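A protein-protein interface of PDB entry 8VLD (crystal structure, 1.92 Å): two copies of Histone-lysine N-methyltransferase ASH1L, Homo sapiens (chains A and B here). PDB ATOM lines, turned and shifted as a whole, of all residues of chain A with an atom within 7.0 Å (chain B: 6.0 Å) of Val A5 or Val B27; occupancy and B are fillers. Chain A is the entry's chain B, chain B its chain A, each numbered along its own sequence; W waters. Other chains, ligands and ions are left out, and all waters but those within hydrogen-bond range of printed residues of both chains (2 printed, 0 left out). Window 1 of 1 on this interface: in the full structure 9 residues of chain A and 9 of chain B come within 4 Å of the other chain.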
ATOM      1  N   GLY A   1      21.381  16.805 -12.865  1.00  0.00           N
ATOM      2  CA  GLY A   1      20.302  17.696 -13.256  1.00  0.00           C
ATOM      3  C   GLY A   1      20.768  19.113 -13.526  1.00  0.00           C
ATOM      4  O   GLY A   1      21.936  19.429 -13.299  1.00  0.00           O
ATOM      5  N   PRO A   2      19.852  19.968 -13.997  1.00  0.00           N
ATOM      6  CA  PRO A   2      20.252  21.310 -14.454  1.00  0.00           C
ATOM      7  C   PRO A   2      21.023  22.120 -13.432  1.00  0.00           C
ATOM      8  O   PRO A   2      21.813  22.991 -13.815  1.00  0.00           O
ATOM      9  CB  PRO A   2      18.907  21.967 -14.791  1.00  0.00           C
ATOM     10  CG  PRO A   2      18.034  20.822 -15.155  1.00  0.00           C
ATOM     11  CD  PRO A   2      18.425  19.705 -14.242  1.00  0.00           C
ATOM     12  N   LEU A   3      20.832  21.863 -12.143  1.00  0.00           N
ATOM     13  CA  LEU A   3      21.548  22.614 -11.126  1.00  0.00           C
ATOM     14  C   LEU A   3      22.712  21.825 -10.530  1.00  0.00           C
ATOM     15  O   LEU A   3      23.602  22.503  -9.915  1.00  0.00           O
ATOM     16  CB  LEU A   3      20.614  22.893  -9.936  1.00  0.00           C
ATOM     17  CG  LEU A   3      20.029  21.756  -9.088  1.00  0.00           C
ATOM     18  CD1 LEU A   3      21.024  21.280  -8.027  1.00  0.00           C
ATOM     19  CD2 LEU A   3      18.690  22.149  -8.468  1.00  0.00           C
ATOM     20  N   ASP A   4      23.029  20.661 -11.091  1.00  0.00           N
ATOM     21  CA  ASP A   4      24.229  19.914 -10.744  1.00  0.00           C
ATOM     22  C   ASP A   4      25.315  20.273 -11.748  1.00  0.00           C
ATOM     23  O   ASP A   4      25.182  19.975 -12.940  1.00  0.00           O
ATOM     24  CB  ASP A   4      23.968  18.408 -10.778  1.00  0.00           C
ATOM     25  CG  ASP A   4      22.946  17.966  -9.756  1.00  0.00           C
ATOM     26  OD1 ASP A   4      23.028  18.428  -8.600  1.00  0.00           O
ATOM     27  OD2 ASP A   4      22.066  17.153 -10.113  1.00  0.00           O
ATOM     28  N   VAL A   5      26.382  20.903 -11.277  1.00  0.00           N
ATOM     29  CA  VAL A   5      27.448  21.366 -12.156  1.00  0.00           C
ATOM     30  C   VAL A   5      28.437  20.233 -12.381  1.00  0.00           C
ATOM     31  O   VAL A   5      29.026  19.714 -11.426  1.00  0.00           O
ATOM     32  CB  VAL A   5      28.152  22.598 -11.576  1.00  0.00           C
ATOM     33  CG1 VAL A   5      29.312  22.996 -12.471  1.00  0.00           C
ATOM     34  CG2 VAL A   5      27.156  23.740 -11.441  1.00  0.00           C
ATOM     35  N   ILE A   6      28.629  19.861 -13.642  1.00  0.00           N
ATOM     36  CA  ILE A   6      29.647  18.897 -14.039  1.00  0.00           C
ATOM     37  C   ILE A   6      30.872  19.685 -14.495  1.00  0.00           C
ATOM     38  O   ILE A   6      30.799  20.452 -15.463  1.00  0.00           O
ATOM     39  CB  ILE A   6      29.135  17.968 -15.151  1.00  0.00           C
ATOM     40  CG1 ILE A   6      27.983  17.097 -14.643  1.00  0.00           C
ATOM     41  CG2 ILE A   6      30.250  17.075 -15.652  1.00  0.00           C
ATOM     42  CD1 ILE A   6      27.255  16.358 -15.762  1.00  0.00           C
ATOM     43  N   ARG A   7      31.997  19.518 -13.795  1.00  0.00           N
ATOM     44  CA  ARG A   7      33.264  20.117 -14.223  1.00  0.00           C
ATOM     45  C   ARG A   7      34.364  19.085 -14.003  1.00  0.00           C
ATOM     46  O   ARG A   7      35.047  19.089 -12.977  1.00  0.00           O
ATOM     47  CB  ARG A   7      33.583  21.416 -13.488  1.00  0.00           C
ATOM     48  CG  ARG A   7      34.745  22.160 -14.136  1.00  0.00           C
ATOM     49  CD  ARG A   7      35.406  23.172 -13.209  1.00  0.00           C
ATOM     50  NE  ARG A   7      36.008  22.559 -12.025  1.00  0.00           N
ATOM     51  CZ  ARG A   7      37.098  21.793 -12.038  1.00  0.00           C
ATOM     52  NH1 ARG A   7      37.729  21.522 -13.177  1.00  0.00           N
ATOM     53  NH2 ARG A   7      37.563  21.295 -10.902  1.00  0.00           N
ATOM     54  N   CYS A   8      34.539  18.207 -14.983  1.00  0.00           N
ATOM     55  CA  CYS A   8      35.582  17.199 -14.933  1.00  0.00           C
ATOM     56  C   CYS A   8      36.780  17.658 -15.754  1.00  0.00           C
ATOM     57  O   CYS A   8      36.671  18.518 -16.632  1.00  0.00           O
ATOM     58  CB  CYS A   8      35.059  15.851 -15.441  1.00  0.00           C
ATOM     59  SG  CYS A   8      36.165  14.465 -15.121  1.00  0.00           S
ATOM     60  N   TYR A  13      30.708  17.788 -20.652  1.00  0.00           N
ATOM     61  CA  TYR A  13      29.550  18.007 -19.790  1.00  0.00           C
ATOM     62  C   TYR A  13      28.542  16.888 -20.025  1.00  0.00           C
ATOM     63  O   TYR A  13      27.520  17.055 -20.694  1.00  0.00           O
ATOM     64  CB  TYR A  13      28.933  19.376 -20.047  1.00  0.00           C
ATOM     65  CG  TYR A  13      28.211  19.910 -18.839  1.00  0.00           C
ATOM     66  CD1 TYR A  13      26.960  19.424 -18.484  1.00  0.00           C
ATOM     67  CD2 TYR A  13      28.790  20.880 -18.036  1.00  0.00           C
ATOM     68  CE1 TYR A  13      26.301  19.901 -17.368  1.00  0.00           C
ATOM     69  CE2 TYR A  13      28.143  21.365 -16.927  1.00  0.00           C
ATOM     70  CZ  TYR A  13      26.898  20.874 -16.595  1.00  0.00           C
ATOM     71  OH  TYR A  13      26.259  21.359 -15.483  1.00  0.00           O
ATOM     72  N   MET A  19      30.232   8.892 -10.750  1.00  0.00           N
ATOM     73  CA  MET A  19      30.604  10.290 -10.650  1.00  0.00           C
ATOM     74  C   MET A  19      30.725  10.663  -9.180  1.00  0.00           C
ATOM     75  O   MET A  19      30.070  10.067  -8.321  1.00  0.00           O
ATOM     76  CB  MET A  19      29.572  11.165 -11.371  1.00  0.00           C
ATOM     77  CG  MET A  19      29.810  11.213 -12.876  1.00  0.00           C
ATOM     78  SD  MET A  19      28.818  12.411 -13.769  1.00  0.00           S
ATOM     79  CE  MET A  19      29.927  13.814 -13.765  1.00  0.00           C
ATOM     80  N   GLN A  21      31.418  14.010  -6.247  1.00  0.00           N
ATOM     81  CA  GLN A  21      31.240  15.436  -6.011  1.00  0.00           C
ATOM     82  C   GLN A  21      32.358  15.967  -5.126  1.00  0.00           C
ATOM     83  O   GLN A  21      32.689  15.361  -4.100  1.00  0.00           O
ATOM     84  CB  GLN A  21      29.881  15.710  -5.367  1.00  0.00           C
ATOM     85  CG  GLN A  21      29.618  17.177  -5.088  1.00  0.00           C
ATOM     86  CD  GLN A  21      28.205  17.431  -4.617  1.00  0.00           C
ATOM     87  OE1 GLN A  21      27.704  16.751  -3.722  1.00  0.00           O
ATOM     88  NE2 GLN A  21      27.547  18.408  -5.228  1.00  0.00           N
ATOM     89  N   CYS A  25      33.597  22.681  -3.536  1.00  0.00           N
ATOM     90  CA  CYS A  25      32.992  23.520  -4.567  1.00  0.00           C
ATOM     91  C   CYS A  25      31.776  22.891  -5.244  1.00  0.00           C
ATOM     92  O   CYS A  25      31.177  23.533  -6.111  1.00  0.00           O
ATOM     93  CB  CYS A  25      34.043  23.916  -5.614  1.00  0.00           C
ATOM     94  SG  CYS A  25      34.528  22.633  -6.772  1.00  0.00           S
ATOM     95  N   MET A  26      31.386  21.671  -4.861  1.00  0.00           N
ATOM     96  CA  MET A  26      30.179  20.968  -5.307  1.00  0.00           C
ATOM     97  C   MET A  26      30.198  20.467  -6.749  1.00  0.00           C
ATOM     98  O   MET A  26      29.198  19.891  -7.181  1.00  0.00           O
ATOM     99  CB  MET A  26      28.900  21.806  -5.135  1.00  0.00           C
ATOM    100  CG  MET A  26      28.517  22.179  -3.711  1.00  0.00           C
ATOM    101  SD  MET A  26      28.593  20.785  -2.567  1.00  0.00           S
ATOM    102  CE  MET A  26      30.175  21.029  -1.796  1.00  0.00           C
ATOM    103  N   VAL A  27      31.283  20.642  -7.506  1.00  0.00           N
ATOM    104  CA  VAL A  27      31.280  20.147  -8.879  1.00  0.00           C
ATOM    105  C   VAL A  27      31.376  18.626  -8.895  1.00  0.00           C
ATOM    106  O   VAL A  27      31.930  17.998  -7.981  1.00  0.00           O
ATOM    107  CB  VAL A  27      32.407  20.776  -9.717  1.00  0.00           C
ATOM    108  CG1 VAL A  27      32.313  22.299  -9.683  1.00  0.00           C
ATOM    109  CG2 VAL A  27      33.764  20.300  -9.243  1.00  0.00           C
ATOM    110  N   TRP A  28      30.826  18.029  -9.948  1.00  0.00           N
ATOM    111  CA  TRP A  28      30.838  16.589 -10.165  1.00  0.00           C
ATOM    112  C   TRP A  28      31.867  16.243 -11.229  1.00  0.00           C
ATOM    113  O   TRP A  28      32.013  16.959 -12.223  1.00  0.00           O
ATOM    114  CB  TRP A  28      29.467  16.086 -10.614  1.00  0.00           C
ATOM    115  CG  TRP A  28      28.421  16.200  -9.578  1.00  0.00           C
ATOM    116  CD1 TRP A  28      27.608  17.271  -9.350  1.00  0.00           C
ATOM    117  CD2 TRP A  28      28.042  15.196  -8.635  1.00  0.00           C
ATOM    118  NE1 TRP A  28      26.754  17.001  -8.308  1.00  0.00           N
ATOM    119  CE2 TRP A  28      27.003  15.732  -7.852  1.00  0.00           C
ATOM    120  CE3 TRP A  28      28.491  13.897  -8.368  1.00  0.00           C
ATOM    121  CZ2 TRP A  28      26.399  15.012  -6.823  1.00  0.00           C
ATOM    122  CZ3 TRP A  28      27.892  13.188  -7.349  1.00  0.00           C
ATOM    123  CH2 TRP A  28      26.858  13.746  -6.588  1.00  0.00           C
ATOM    124  N   GLN A  29      32.575  15.138 -11.018  1.00  0.00           N
ATOM    125  CA  GLN A  29      33.594  14.680 -11.947  1.00  0.00           C
ATOM    126  C   GLN A  29      33.423  13.183 -12.143  1.00  0.00           C
ATOM    127  O   GLN A  29      32.818  12.504 -11.313  1.00  0.00           O
ATOM    128  CB  GLN A  29      34.999  15.006 -11.425  1.00  0.00           C
ATOM    129  CG  GLN A  29      35.114  16.407 -10.806  1.00  0.00           C
ATOM    130  CD  GLN A  29      36.541  16.872 -10.667  1.00  0.00           C
ATOM    131  OE1 GLN A  29      37.307  16.340  -9.856  1.00  0.00           O
ATOM    132  NE2 GLN A  29      36.912  17.876 -11.453  1.00  0.00           N
ATOM    133  N   VAL B   5      33.191  28.682  -8.822  1.00  0.00           N
ATOM    134  CA  VAL B   5      33.410  27.688  -9.867  1.00  0.00           C
ATOM    135  C   VAL B   5      33.469  28.393 -11.215  1.00  0.00           C
ATOM    136  O   VAL B   5      32.518  29.076 -11.609  1.00  0.00           O
ATOM    137  CB  VAL B   5      32.303  26.625  -9.856  1.00  0.00           C
ATOM    138  CG1 VAL B   5      32.474  25.675 -11.023  1.00  0.00           C
ATOM    139  CG2 VAL B   5      32.301  25.876  -8.527  1.00  0.00           C
ATOM    140  N   ILE B   6      34.579  28.226 -11.928  1.00  0.00           N
ATOM    141  CA  ILE B   6      34.714  28.703 -13.301  1.00  0.00           C
ATOM    142  C   ILE B   6      34.416  27.529 -14.226  1.00  0.00           C
ATOM    143  O   ILE B   6      35.070  26.486 -14.140  1.00  0.00           O
ATOM    144  CB  ILE B   6      36.118  29.270 -13.567  1.00  0.00           C
ATOM    145  CG1 ILE B   6      36.393  30.496 -12.693  1.00  0.00           C
ATOM    146  CG2 ILE B   6      36.274  29.634 -15.036  1.00  0.00           C
ATOM    147  CD1 ILE B   6      37.856  30.905 -12.685  1.00  0.00           C
ATOM    148  N   ARG B   7      33.428  27.681 -15.110  1.00  0.00           N
ATOM    149  CA  ARG B   7      33.153  26.658 -16.126  1.00  0.00           C
ATOM    150  C   ARG B   7      32.737  27.375 -17.406  1.00  0.00           C
ATOM    151  O   ARG B   7      31.547  27.574 -17.656  1.00  0.00           O
ATOM    152  CB  ARG B   7      32.085  25.665 -15.692  1.00  0.00           C
ATOM    153  CG  ARG B   7      32.013  24.469 -16.636  1.00  0.00           C
ATOM    154  CD  ARG B   7      30.672  23.761 -16.586  1.00  0.00           C
ATOM    155  NE  ARG B   7      29.562  24.642 -16.948  1.00  0.00           N
ATOM    156  CZ  ARG B   7      29.279  25.018 -18.193  1.00  0.00           C
ATOM    157  NH1 ARG B   7      30.027  24.601 -19.206  1.00  0.00           N
ATOM    158  NH2 ARG B   7      28.246  25.820 -18.428  1.00  0.00           N
ATOM    159  N   ILE B  20      31.142  36.622 -15.998  1.00  0.00           N
ATOM    160  CA  ILE B  20      29.728  36.748 -15.681  1.00  0.00           C
ATOM    161  C   ILE B  20      29.243  35.427 -15.099  1.00  0.00           C
ATOM    162  O   ILE B  20      29.733  34.351 -15.458  1.00  0.00           O
ATOM    163  CB  ILE B  20      28.924  37.141 -16.940  1.00  0.00           C
ATOM    164  CG1 ILE B  20      27.465  37.422 -16.600  1.00  0.00           C
ATOM    165  CG2 ILE B  20      29.031  36.046 -17.988  1.00  0.00           C
ATOM    166  CD1 ILE B  20      26.751  38.232 -17.669  1.00  0.00           C
ATOM    167  N   GLN B  21      28.275  35.511 -14.193  1.00  0.00           N
ATOM    168  CA  GLN B  21      27.792  34.351 -13.457  1.00  0.00           C
ATOM    169  C   GLN B  21      26.426  33.911 -13.965  1.00  0.00           C
ATOM    170  O   GLN B  21      25.538  34.743 -14.189  1.00  0.00           O
ATOM    171  CB  GLN B  21      27.714  34.656 -11.963  1.00  0.00           C
ATOM    172  CG  GLN B  21      27.245  33.478 -11.142  1.00  0.00           C
ATOM    173  CD  GLN B  21      27.386  33.720  -9.662  1.00  0.00           C
ATOM    174  OE1 GLN B  21      27.026  34.783  -9.158  1.00  0.00           O
ATOM    175  NE2 GLN B  21      27.907  32.731  -8.954  1.00  0.00           N
ATOM    176  N   CYS B  22      26.268  32.603 -14.149  1.00  0.00           N
ATOM    177  CA  CYS B  22      24.963  32.036 -14.457  1.00  0.00           C
ATOM    178  C   CYS B  22      24.015  32.202 -13.275  1.00  0.00           C
ATOM    179  O   CYS B  22      24.356  31.857 -12.138  1.00  0.00           O
ATOM    180  CB  CYS B  22      25.103  30.560 -14.812  1.00  0.00           C
ATOM    181  SG  CYS B  22      23.566  29.745 -15.249  1.00  0.00           S
ATOM    182  N   LYS B  24      21.259  30.583 -12.584  1.00  0.00           N
ATOM    183  CA  LYS B  24      20.899  29.261 -12.042  1.00  0.00           C
ATOM    184  C   LYS B  24      22.044  28.527 -11.352  1.00  0.00           C
ATOM    185  O   LYS B  24      22.044  28.380 -10.130  1.00  0.00           O
ATOM    186  CB  LYS B  24      20.303  28.394 -13.158  1.00  0.00           C
ATOM    187  CG  LYS B  24      19.020  28.910 -13.759  1.00  0.00           C
ATOM    188  CD  LYS B  24      17.850  28.709 -12.765  1.00  0.00           C
ATOM    189  CE  LYS B  24      17.507  29.829 -11.861  1.00  0.00           C
ATOM    190  NZ  LYS B  24      16.300  29.430 -11.089  1.00  0.00           N
ATOM    191  N   CYS B  25      23.018  28.049 -12.116  1.00  0.00           N
ATOM    192  CA  CYS B  25      23.986  27.101 -11.585  1.00  0.00           C
ATOM    193  C   CYS B  25      25.211  27.758 -10.970  1.00  0.00           C
ATOM    194  O   CYS B  25      26.078  27.045 -10.456  1.00  0.00           O
ATOM    195  CB  CYS B  25      24.413  26.110 -12.674  1.00  0.00           C
ATOM    196  SG  CYS B  25      25.501  26.769 -13.933  1.00  0.00           S
ATOM    197  N   MET B  26      25.302  29.087 -10.994  1.00  0.00           N
ATOM    198  CA  MET B  26      26.323  29.891 -10.318  1.00  0.00           C
ATOM    199  C   MET B  26      27.734  29.767 -10.889  1.00  0.00           C
ATOM    200  O   MET B  26      28.643  30.402 -10.344  1.00  0.00           O
ATOM    201  CB  MET B  26      26.410  29.604  -8.809  1.00  0.00           C
ATOM    202  CG  MET B  26      25.078  29.479  -8.093  1.00  0.00           C
ATOM    203  SD  MET B  26      23.957  30.793  -8.589  1.00  0.00           S
ATOM    204  CE  MET B  26      24.501  32.085  -7.480  1.00  0.00           C
ATOM    205  N   VAL B  27      27.960  28.997 -11.956  1.00  0.00           N
ATOM    206  CA  VAL B  27      29.307  28.975 -12.533  1.00  0.00           C
ATOM    207  C   VAL B  27      29.617  30.318 -13.189  1.00  0.00           C
ATOM    208  O   VAL B  27      28.726  31.074 -13.596  1.00  0.00           O
ATOM    209  CB  VAL B  27      29.489  27.826 -13.536  1.00  0.00           C
ATOM    210  CG1 VAL B  27      29.139  26.505 -12.897  1.00  0.00           C
ATOM    211  CG2 VAL B  27      28.666  28.062 -14.791  1.00  0.00           C
ATOM    212  N   TRP B  28      30.912  30.605 -13.303  1.00  0.00           N
ATOM    213  CA  TRP B  28      31.416  31.821 -13.925  1.00  0.00           C
ATOM    214  C   TRP B  28      32.008  31.500 -15.290  1.00  0.00           C
ATOM    215  O   TRP B  28      32.609  30.442 -15.493  1.00  0.00           O
ATOM    216  CB  TRP B  28      32.486  32.486 -13.054  1.00  0.00           C
ATOM    217  CG  TRP B  28      31.962  33.035 -11.782  1.00  0.00           C
ATOM    218  CD1 TRP B  28      31.803  32.365 -10.600  1.00  0.00           C
ATOM    219  CD2 TRP B  28      31.540  34.380 -11.540  1.00  0.00           C
ATOM    220  NE1 TRP B  28      31.295  33.212  -9.643  1.00  0.00           N
ATOM    221  CE2 TRP B  28      31.125  34.455 -10.196  1.00  0.00           C
ATOM    222  CE3 TRP B  28      31.461  35.528 -12.335  1.00  0.00           C
ATOM    223  CZ2 TRP B  28      30.645  35.633  -9.628  1.00  0.00           C
ATOM    224  CZ3 TRP B  28      30.986  36.694 -11.769  1.00  0.00           C
ATOM    225  CH2 TRP B  28      30.583  36.738 -10.431  1.00  0.00           C
ATOM    226  N   GLN B  29      31.843  32.433 -16.222  1.00  0.00           N
ATOM    227  CA  GLN B  29      32.279  32.262 -17.601  1.00  0.00           C
ATOM    228  C   GLN B  29      32.856  33.581 -18.094  1.00  0.00           C
ATOM    229  O   GLN B  29      32.471  34.648 -17.617  1.00  0.00           O
ATOM    230  CB  GLN B  29      31.110  31.832 -18.499  1.00  0.00           C
ATOM    231  CG  GLN B  29      30.261  30.690 -17.928  1.00  0.00           C
ATOM    232  CD  GLN B  29      29.426  29.994 -18.980  1.00  0.00           C
ATOM    233  OE1 GLN B  29      28.511  30.587 -19.557  1.00  0.00           O
ATOM    234  NE2 GLN B  29      29.726  28.724 -19.227  1.00  0.00           N
ATOM    235  N   TYR B  43      21.589  36.348 -16.937  1.00  0.00           N
ATOM    236  CA  TYR B  43      22.502  35.481 -17.671  1.00  0.00           C
ATOM    237  C   TYR B  43      22.279  34.029 -17.285  1.00  0.00           C
ATOM    238  O   TYR B  43      22.129  33.715 -16.103  1.00  0.00           O
ATOM    239  CB  TYR B  43      23.972  35.838 -17.418  1.00  0.00           C
ATOM    240  CG  TYR B  43      24.884  35.009 -18.286  1.00  0.00           C
ATOM    241  CD1 TYR B  43      24.949  35.241 -19.652  1.00  0.00           C
ATOM    242  CD2 TYR B  43      25.635  33.957 -17.759  1.00  0.00           C
ATOM    243  CE1 TYR B  43      25.750  34.487 -20.466  1.00  0.00           C
ATOM    244  CE2 TYR B  43      26.447  33.194 -18.573  1.00  0.00           C
ATOM    245  CZ  TYR B  43      26.497  33.467 -19.927  1.00  0.00           C
ATOM    246  OH  TYR B  43      27.288  32.725 -20.762  1.00  0.00           O
ATOM    247  N   CYS B  45      24.131  30.145 -18.460  1.00  0.00           N
ATOM    248  CA  CYS B  45      25.217  29.521 -19.199  1.00  0.00           C
ATOM    249  C   CYS B  45      24.663  28.653 -20.327  1.00  0.00           C
ATOM    250  O   CYS B  45      23.454  28.456 -20.469  1.00  0.00           O
ATOM    251  CB  CYS B  45      26.094  28.702 -18.256  1.00  0.00           C
ATOM    252  SG  CYS B  45      25.286  27.219 -17.634  1.00  0.00           S
HETATM  253  O   HOH W   1      24.804  24.980  -8.661  1.00  0.00           O
HETATM  254  O   HOH W   2      27.193  24.409 -15.276  1.00  0.00           O
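Among the printed residues, merely in contact across the chains: Val A5 with Cys B25, Val A5 with Val B27, Ile A6 with Arg B7, Arg A7 with Ile B6, Tyr A13 with Arg B7, Cys A25 with Val B5 and Val A27 with Val B5.
Of the 16 printed residues of chain A, 6 touch a printed residue of chain B.
Printed residues of chain B that touch a printed residue of chain A: Val B5, Ile B6, Arg B7, Cys B25 and Val B27.
Among the printed residues, no Asp or Glu carboxylate lies within 4 Å of a Lys or Arg side-chain nitrogen of the other chain.
Of chain B, only Cys B25 (3.6 Å) and Val B27 (3.5 Å) come within 4 Å of Val A5.
Val B27 touches one residue of chain A.
Of the printed residues of chain B, Cys A25 touches Val B5.
Printed residues of chain A within 4 Å of Ile B6: Arg A7 (3.5 Å).
Of the printed residues of chain A, Val B5 touches Cys A25 (3.5 Å) and Val A27 (3.6 Å).
Of the printed residues of chain A, Cys B25 touches Val A5 (3.6 Å).
Met B26 touches none of the printed residues of chain A.
Val A5 touches Cys B25, and with the chains exchanged Cys A25 touches Val B5.
Val A5 touches Val B27, and with the chains exchanged Val A27 touches Val B5.
Ile A6 touches Arg B7, and with the chains exchanged Arg A7 touches Ile B6.
Positions printed for both chains: 5, 6, 7, 21, 25, 26, 27, 28 and 29.
Of the 7 pairs that touch across the chains among the printed residues, 6 have their exchanged pair printed and touching as well.
The backbone carbonyl oxygen (O) of Val B5 is in hydrogen-bond range of the backbone NH (N) of Trp B28 (2.8 Å).
The backbone carbonyl oxygen (O) of Arg B7 is in hydrogen-bond range of the side-chain amide nitrogen (NE2) of Gln B29, 2.7 Å away.
SG of Cys B45 lies close to NH2 of Arg B7, at 3.4 Å.
The backbone carbonyl oxygen (O) of Val B27 sits at hydrogen-bond distance from the backbone NH (N) of Cys B22 (2.9 Å).
O of Val A5 sits at hydrogen-bond distance from N of Trp A28 (2.9 Å).
The backbone carbonyl oxygen (O) of Trp A28 lies within hydrogen-bond range of the backbone NH (N) of Arg A7, 3.0 Å away.
Water W2 lies within hydrogen-bond range of NE of Arg B7 (2.9 Å) and OH of Tyr A13 (3.2 Å).
Water W1 lies within hydrogen-bond range of the backbone carbonyl oxygen (O) of Cys B25 (3.0 Å) and the backbone carbonyl oxygen (O) of Leu A3 (3.0 Å).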
